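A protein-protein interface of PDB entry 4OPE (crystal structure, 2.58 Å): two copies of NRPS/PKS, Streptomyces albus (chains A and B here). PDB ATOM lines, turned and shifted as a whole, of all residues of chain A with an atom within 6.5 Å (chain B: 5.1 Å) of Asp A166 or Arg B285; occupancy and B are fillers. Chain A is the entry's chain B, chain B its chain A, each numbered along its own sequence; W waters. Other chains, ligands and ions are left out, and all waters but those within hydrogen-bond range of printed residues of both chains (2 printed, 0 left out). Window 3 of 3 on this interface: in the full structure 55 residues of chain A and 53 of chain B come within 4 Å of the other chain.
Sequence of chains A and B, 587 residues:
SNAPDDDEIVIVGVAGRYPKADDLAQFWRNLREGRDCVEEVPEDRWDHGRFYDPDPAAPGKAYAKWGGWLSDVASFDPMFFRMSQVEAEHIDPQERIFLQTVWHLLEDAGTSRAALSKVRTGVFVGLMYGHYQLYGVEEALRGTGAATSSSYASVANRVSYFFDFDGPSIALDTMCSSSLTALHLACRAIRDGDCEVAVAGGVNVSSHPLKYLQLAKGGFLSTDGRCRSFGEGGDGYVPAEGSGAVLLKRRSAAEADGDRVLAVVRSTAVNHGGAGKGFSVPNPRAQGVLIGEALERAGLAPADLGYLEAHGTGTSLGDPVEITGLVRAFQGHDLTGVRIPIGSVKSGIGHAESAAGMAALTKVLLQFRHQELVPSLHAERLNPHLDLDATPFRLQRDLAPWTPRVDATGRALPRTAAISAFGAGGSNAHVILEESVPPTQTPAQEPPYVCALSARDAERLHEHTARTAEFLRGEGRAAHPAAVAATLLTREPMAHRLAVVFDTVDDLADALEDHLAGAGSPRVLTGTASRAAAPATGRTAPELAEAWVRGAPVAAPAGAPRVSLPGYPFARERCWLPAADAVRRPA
The backbone carbonyl oxygen (O) of Ala B286 sits at hydrogen-bond distance from the side-chain amide nitrogen (ND2) of Asn B271, 3.1 Å away.
ND1 of His B272 lies within hydrogen-bond range of N of Gly B274 (3.1 Å).
The side-chain amide oxygen (OD1) of Asn B283 is in hydrogen-bond range of the backbone NH (N) of Arg B285 (2.8 Å).
The backbone NH of Asp A166 sits at hydrogen-bond distance from the backbone carbonyl oxygen of Thr A121, 3.4 Å away.
O of Thr A121 sits at hydrogen-bond distance from N of Gly A167 (2.9 Å).
The backbone NH of Phe A165 is in hydrogen-bond range of the backbone carbonyl oxygen of Ser A160, 3.0 Å away.
Among the printed residues, pairs that only touch across the chains: Arg A120 with Val B289, Ser A160 with His B272, Ser A160 with Gly B274, Asp A164 with Gly B274, Phe A165 with His B272, Phe A165 with Gly B274, Asp A166 with Asn B271 and Gly A167 with Asn B271.
Of the 12 printed residues of chain B, 5 touch a printed residue of chain A.
Printed residues of chain B that touch a printed residue of chain A: Asn B271, His B272, Gly B274, Arg B285 and Val B289.
Hydrophobic or aromatic side chains of chain B that line the printed part of chain A: His B272 and Val B289.
Among the printed residues, Asp or Glu carboxylates within 4 Å of a Lys or Arg side-chain nitrogen of the other chain: Asp A166 with Arg B285 (3.1 Å).
Water W2 lies within hydrogen-bond range of NH2 of Arg B285 (2.9 Å), O of Gly B273 (3.0 Å) and OD1 of Asp A164 (3.2 Å).
Water W1 lies within hydrogen-bond range of the backbone carbonyl oxygen of Asp A166 (2.9 Å), the guanidinium group of Arg A120 (3.1 Å) and the side-chain amide nitrogen of Asn B271 (3.2 Å).
Of chain B, only Asn B271, His B272 and Arg B285 come within 4 Å of Asp A166.
Printed residues of chain B within 4 Å of Phe A165: His B272 (3.7 Å) and Gly B274 (3.7 Å).
Printed residues of chain B within 4 Å of Asp A164: Gly B274 (3.6 Å).
Gln B287 touches none of the printed residues of chain A.
Pro A168 touches none of the printed residues of chain B.
The nearest residue of chain A that does not touch Arg B285 is Asp A164 (5.9 Å).
The backbone carbonyl oxygen (O) of Asp A166 lies within hydrogen-bond range of the backbone NH (N) of His B272, 3.2 Å away.
The backbone NH of His B272 lies within hydrogen-bond range of the backbone carbonyl oxygen of Gly A167, at 3.1 Å.
The guanidinium group of Arg B285 lies within salt-bridge range of the side-chain carboxylate of Asp A166 (3.1 Å).
No position is printed for both chains.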
ATOM      1  N   SER A 117      13.179  11.866   1.973  1.00  0.00           N
ATOM      2  CA  SER A 117      13.966  12.772   1.151  1.00  0.00           C
ATOM      3  C   SER A 117      15.421  12.334   1.011  1.00  0.00           C
ATOM      4  O   SER A 117      16.095  12.782   0.104  1.00  0.00           O
ATOM      5  CB  SER A 117      13.943  14.180   1.737  1.00  0.00           C
ATOM      6  OG  SER A 117      14.946  14.339   2.726  1.00  0.00           O
ATOM      7  N   VAL A 119      16.464   9.072   0.937  1.00  0.00           N
ATOM      8  CA  VAL A 119      16.555   7.889   0.104  1.00  0.00           C
ATOM      9  C   VAL A 119      16.063   8.236  -1.279  1.00  0.00           C
ATOM     10  O   VAL A 119      15.414   9.234  -1.498  1.00  0.00           O
ATOM     11  CB  VAL A 119      15.767   6.686   0.668  1.00  0.00           C
ATOM     12  CG1 VAL A 119      16.464   6.151   1.911  1.00  0.00           C
ATOM     13  CG2 VAL A 119      14.327   7.048   0.983  1.00  0.00           C
ATOM     14  N   ARG A 120      16.418   7.412  -2.228  1.00  0.00           N
ATOM     15  CA  ARG A 120      15.998   7.615  -3.600  1.00  0.00           C
ATOM     16  C   ARG A 120      14.738   6.814  -3.844  1.00  0.00           C
ATOM     17  O   ARG A 120      14.781   5.589  -3.756  1.00  0.00           O
ATOM     18  CB  ARG A 120      17.090   7.130  -4.498  1.00  0.00           C
ATOM     19  CG  ARG A 120      17.027   7.650  -5.900  1.00  0.00           C
ATOM     20  CD  ARG A 120      18.252   7.101  -6.547  1.00  0.00           C
ATOM     21  NE  ARG A 120      18.637   7.861  -7.696  1.00  0.00           N
ATOM     22  CZ  ARG A 120      19.723   7.589  -8.389  1.00  0.00           C
ATOM     23  NH1 ARG A 120      20.502   6.577  -8.024  1.00  0.00           N
ATOM     24  NH2 ARG A 120      20.013   8.320  -9.455  1.00  0.00           N
ATOM     25  N   THR A 121      13.625   7.494  -4.112  1.00  0.00           N
ATOM     26  CA  THR A 121      12.319   6.829  -4.257  1.00  0.00           C
ATOM     27  C   THR A 121      11.832   6.872  -5.709  1.00  0.00           C
ATOM     28  O   THR A 121      11.853   7.935  -6.331  1.00  0.00           O
ATOM     29  CB  THR A 121      11.240   7.462  -3.346  1.00  0.00           C
ATOM     30  OG1 THR A 121      11.710   7.482  -1.993  1.00  0.00           O
ATOM     31  CG2 THR A 121       9.950   6.636  -3.409  1.00  0.00           C
ATOM     32  N   GLY A 122      11.413   5.714  -6.224  1.00  0.00           N
ATOM     33  CA  GLY A 122      10.876   5.582  -7.564  1.00  0.00           C
ATOM     34  C   GLY A 122       9.367   5.366  -7.537  1.00  0.00           C
ATOM     35  O   GLY A 122       8.821   5.019  -6.516  1.00  0.00           O
ATOM     36  N   SER A 160       5.750  11.954  -8.645  1.00  0.00           N
ATOM     37  CA  SER A 160       7.179  12.133  -8.418  1.00  0.00           C
ATOM     38  C   SER A 160       7.517  13.597  -8.129  1.00  0.00           C
ATOM     39  O   SER A 160       8.444  13.896  -7.333  1.00  0.00           O
ATOM     40  CB  SER A 160       8.009  11.627  -9.609  1.00  0.00           C
ATOM     41  OG  SER A 160       7.827  10.233  -9.814  1.00  0.00           O
ATOM     42  N   ASP A 164       8.548  14.648  -4.324  1.00  0.00           N
ATOM     43  CA  ASP A 164      10.008  14.753  -4.440  1.00  0.00           C
ATOM     44  C   ASP A 164      10.690  13.380  -4.494  1.00  0.00           C
ATOM     45  O   ASP A 164      11.692  13.149  -3.858  1.00  0.00           O
ATOM     46  CB  ASP A 164      10.584  15.591  -3.289  1.00  0.00           C
ATOM     47  CG  ASP A 164      11.988  16.137  -3.578  1.00  0.00           C
ATOM     48  OD1 ASP A 164      12.300  16.473  -4.738  1.00  0.00           O
ATOM     49  OD2 ASP A 164      12.787  16.231  -2.632  1.00  0.00           O
ATOM     50  N   PHE A 165      10.136  12.488  -5.297  1.00  0.00           N
ATOM     51  CA  PHE A 165      10.729  11.205  -5.617  1.00  0.00           C
ATOM     52  C   PHE A 165      11.565  11.350  -6.913  1.00  0.00           C
ATOM     53  O   PHE A 165      11.028  11.671  -7.968  1.00  0.00           O
ATOM     54  CB  PHE A 165       9.589  10.199  -5.814  1.00  0.00           C
ATOM     55  CG  PHE A 165       8.746   9.937  -4.564  1.00  0.00           C
ATOM     56  CD1 PHE A 165       9.182  10.290  -3.290  1.00  0.00           C
ATOM     57  CD2 PHE A 165       7.505   9.318  -4.674  1.00  0.00           C
ATOM     58  CE1 PHE A 165       8.420  10.011  -2.175  1.00  0.00           C
ATOM     59  CE2 PHE A 165       6.731   9.041  -3.548  1.00  0.00           C
ATOM     60  CZ  PHE A 165       7.194   9.373  -2.297  1.00  0.00           C
ATOM     61  N   ASP A 166      12.874  11.137  -6.830  1.00  0.00           N
ATOM     62  CA  ASP A 166      13.789  11.351  -7.979  1.00  0.00           C
ATOM     63  C   ASP A 166      14.423  10.040  -8.546  1.00  0.00           C
ATOM     64  O   ASP A 166      15.415  10.057  -9.276  1.00  0.00           O
ATOM     65  CB  ASP A 166      14.873  12.369  -7.613  1.00  0.00           C
ATOM     66  CG  ASP A 166      15.732  11.916  -6.446  1.00  0.00           C
ATOM     67  OD1 ASP A 166      15.602  10.760  -6.002  1.00  0.00           O
ATOM     68  OD2 ASP A 166      16.551  12.725  -5.954  1.00  0.00           O
ATOM     69  N   GLY A 167      13.844   8.916  -8.167  1.00  0.00           N
ATOM     70  CA  GLY A 167      14.120   7.676  -8.840  1.00  0.00           C
ATOM     71  C   GLY A 167      13.263   7.606 -10.098  1.00  0.00           C
ATOM     72  O   GLY A 167      12.741   8.619 -10.543  1.00  0.00           O
ATOM     73  N   PRO A 168      13.136   6.413 -10.694  1.00  0.00           N
ATOM     74  CA  PRO A 168      12.368   6.245 -11.912  1.00  0.00           C
ATOM     75  C   PRO A 168      10.947   6.668 -11.711  1.00  0.00           C
ATOM     76  O   PRO A 168      10.435   6.551 -10.606  1.00  0.00           O
ATOM     77  CB  PRO A 168      12.426   4.743 -12.151  1.00  0.00           C
ATOM     78  CG  PRO A 168      13.712   4.299 -11.543  1.00  0.00           C
ATOM     79  CD  PRO A 168      13.923   5.207 -10.364  1.00  0.00           C
ATOM     80  N   ASP A 194      18.356   1.260  -9.006  1.00  0.00           N
ATOM     81  CA  ASP A 194      17.771   2.467  -9.622  1.00  0.00           C
ATOM     82  C   ASP A 194      17.171   3.334  -8.515  1.00  0.00           C
ATOM     83  O   ASP A 194      17.089   4.555  -8.626  1.00  0.00           O
ATOM     84  CB  ASP A 194      16.687   2.142 -10.685  1.00  0.00           C
ATOM     85  CG  ASP A 194      17.235   1.418 -11.878  1.00  0.00           C
ATOM     86  OD1 ASP A 194      18.297   1.792 -12.360  1.00  0.00           O
ATOM     87  OD2 ASP A 194      16.618   0.453 -12.345  1.00  0.00           O
ATOM     88  N   ASN B 271      15.832   8.290 -14.198  1.00  0.00           N
ATOM     89  CA  ASN B 271      15.452   8.939 -12.942  1.00  0.00           C
ATOM     90  C   ASN B 271      14.367   9.990 -13.155  1.00  0.00           C
ATOM     91  O   ASN B 271      13.687  10.023 -14.197  1.00  0.00           O
ATOM     92  CB  ASN B 271      16.707   9.510 -12.260  1.00  0.00           C
ATOM     93  CG  ASN B 271      17.184  10.830 -12.853  1.00  0.00           C
ATOM     94  OD1 ASN B 271      16.817  11.232 -13.959  1.00  0.00           O
ATOM     95  ND2 ASN B 271      18.019  11.507 -12.102  1.00  0.00           N
ATOM     96  N   HIS B 272      14.194  10.845 -12.163  1.00  0.00           N
ATOM     97  CA  HIS B 272      13.194  11.899 -12.243  1.00  0.00           C
ATOM     98  C   HIS B 272      13.679  13.169 -11.601  1.00  0.00           C
ATOM     99  O   HIS B 272      14.455  13.130 -10.649  1.00  0.00           O
ATOM    100  CB  HIS B 272      11.892  11.470 -11.569  1.00  0.00           C
ATOM    101  CG  HIS B 272      10.728  12.336 -11.925  1.00  0.00           C
ATOM    102  ND1 HIS B 272      10.326  13.398 -11.154  1.00  0.00           N
ATOM    103  CD2 HIS B 272       9.893  12.312 -12.986  1.00  0.00           C
ATOM    104  CE1 HIS B 272       9.282  13.982 -11.710  1.00  0.00           C
ATOM    105  NE2 HIS B 272       9.003  13.347 -12.830  1.00  0.00           N
ATOM    106  N   GLY B 273      13.185  14.297 -12.097  1.00  0.00           N
ATOM    107  CA  GLY B 273      13.538  15.599 -11.503  1.00  0.00           C
ATOM    108  C   GLY B 273      13.195  15.845 -10.013  1.00  0.00           C
ATOM    109  O   GLY B 273      13.753  16.743  -9.396  1.00  0.00           O
ATOM    110  N   GLY B 274      12.335  15.026  -9.430  1.00  0.00           N
ATOM    111  CA  GLY B 274      11.698  15.328  -8.148  1.00  0.00           C
ATOM    112  C   GLY B 274      10.975  16.672  -8.148  1.00  0.00           C
ATOM    113  O   GLY B 274      10.467  17.095  -9.183  1.00  0.00           O
ATOM    114  N   ASN B 283      15.231  19.906 -14.659  1.00  0.00           N
ATOM    115  CA  ASN B 283      16.037  20.024 -13.483  1.00  0.00           C
ATOM    116  C   ASN B 283      17.472  19.585 -13.767  1.00  0.00           C
ATOM    117  O   ASN B 283      17.752  18.420 -13.952  1.00  0.00           O
ATOM    118  CB  ASN B 283      15.438  19.171 -12.380  1.00  0.00           C
ATOM    119  CG  ASN B 283      16.257  19.205 -11.127  1.00  0.00           C
ATOM    120  OD1 ASN B 283      17.341  19.797 -11.084  1.00  0.00           O
ATOM    121  ND2 ASN B 283      15.752  18.553 -10.084  1.00  0.00           N
ATOM    122  N   PRO B 284      18.407  20.525 -13.732  1.00  0.00           N
ATOM    123  CA  PRO B 284      19.759  20.168 -14.142  1.00  0.00           C
ATOM    124  C   PRO B 284      20.507  19.443 -13.044  1.00  0.00           C
ATOM    125  O   PRO B 284      21.517  18.821 -13.296  1.00  0.00           O
ATOM    126  CB  PRO B 284      20.390  21.531 -14.458  1.00  0.00           C
ATOM    127  CG  PRO B 284      19.704  22.454 -13.533  1.00  0.00           C
ATOM    128  CD  PRO B 284      18.291  21.955 -13.396  1.00  0.00           C
ATOM    129  N   ARG B 285      20.029  19.519 -11.827  1.00  0.00           N
ATOM    130  CA  ARG B 285      20.635  18.720 -10.784  1.00  0.00           C
ATOM    131  C   ARG B 285      20.432  17.240 -11.105  1.00  0.00           C
ATOM    132  O   ARG B 285      21.362  16.443 -11.042  1.00  0.00           O
ATOM    133  CB  ARG B 285      20.025  19.064  -9.421  1.00  0.00           C
ATOM    134  CG  ARG B 285      20.814  18.563  -8.217  1.00  0.00           C
ATOM    135  CD  ARG B 285      19.931  18.172  -7.022  1.00  0.00           C
ATOM    136  NE  ARG B 285      19.733  16.711  -6.947  1.00  0.00           N
ATOM    137  CZ  ARG B 285      18.600  16.047  -7.215  1.00  0.00           C
ATOM    138  NH1 ARG B 285      18.595  14.716  -7.123  1.00  0.00           N
ATOM    139  NH2 ARG B 285      17.472  16.682  -7.566  1.00  0.00           N
ATOM    140  N   ALA B 286      19.215  16.886 -11.473  1.00  0.00           N
ATOM    141  CA  ALA B 286      18.853  15.504 -11.686  1.00  0.00           C
ATOM    142  C   ALA B 286      19.458  14.984 -12.980  1.00  0.00           C
ATOM    143  O   ALA B 286      19.903  13.842 -13.042  1.00  0.00           O
ATOM    144  CB  ALA B 286      17.339  15.373 -11.719  1.00  0.00           C
ATOM    145  N   GLN B 287      19.503  15.824 -14.008  1.00  0.00           N
ATOM    146  CA  GLN B 287      20.203  15.479 -15.208  1.00  0.00           C
ATOM    147  C   GLN B 287      21.653  15.167 -14.906  1.00  0.00           C
ATOM    148  O   GLN B 287      22.222  14.179 -15.393  1.00  0.00           O
ATOM    149  CB  GLN B 287      20.130  16.617 -16.213  1.00  0.00           C
ATOM    150  CG  GLN B 287      18.706  16.906 -16.713  1.00  0.00           C
ATOM    151  CD  GLN B 287      18.619  18.038 -17.752  1.00  0.00           C
ATOM    152  OE1 GLN B 287      19.617  18.483 -18.295  1.00  0.00           O
ATOM    153  NE2 GLN B 287      17.407  18.467 -18.049  1.00  0.00           N
ATOM    154  N   GLY B 288      22.262  16.000 -14.096  1.00  0.00           N
ATOM    155  CA  GLY B 288      23.635  15.776 -13.678  1.00  0.00           C
ATOM    156  C   GLY B 288      23.869  14.442 -12.973  1.00  0.00           C
ATOM    157  O   GLY B 288      24.822  13.696 -13.310  1.00  0.00           O
ATOM    158  N   VAL B 289      23.020  14.141 -12.004  1.00  0.00           N
ATOM    159  CA  VAL B 289      23.104  12.883 -11.299  1.00  0.00           C
ATOM    160  C   VAL B 289      22.987  11.683 -12.244  1.00  0.00           C
ATOM    161  O   VAL B 289      23.819  10.767 -12.224  1.00  0.00           O
ATOM    162  CB  VAL B 289      21.997  12.777 -10.242  1.00  0.00           C
ATOM    163  CG1 VAL B 289      21.995  11.399  -9.599  1.00  0.00           C
ATOM    164  CG2 VAL B 289      22.192  13.869  -9.197  1.00  0.00           C
ATOM    165  N   ARG B 328      27.456  19.759 -14.634  1.00  0.00           N
ATOM    166  CA  ARG B 328      27.336  19.173 -13.316  1.00  0.00           C
ATOM    167  C   ARG B 328      27.780  17.732 -13.267  1.00  0.00           C
ATOM    168  O   ARG B 328      28.310  17.298 -12.260  1.00  0.00           O
ATOM    169  CB  ARG B 328      25.902  19.261 -12.796  1.00  0.00           C
ATOM    170  CG  ARG B 328      25.473  20.681 -12.507  1.00  0.00           C
ATOM    171  CD  ARG B 328      24.162  20.774 -11.732  1.00  0.00           C
ATOM    172  NE  ARG B 328      24.247  19.909 -10.552  1.00  0.00           N
ATOM    173  CZ  ARG B 328      24.327  20.340  -9.295  1.00  0.00           C
ATOM    174  NH1 ARG B 328      24.292  21.639  -9.024  1.00  0.00           N
ATOM    175  NH2 ARG B 328      24.423  19.453  -8.303  1.00  0.00           N
HETATM  176  O   HOH W   1      18.210  10.747  -8.998  1.00  0.00           O
HETATM  177  O   HOH W   2      14.781  17.131  -6.629  1.00  0.00           O
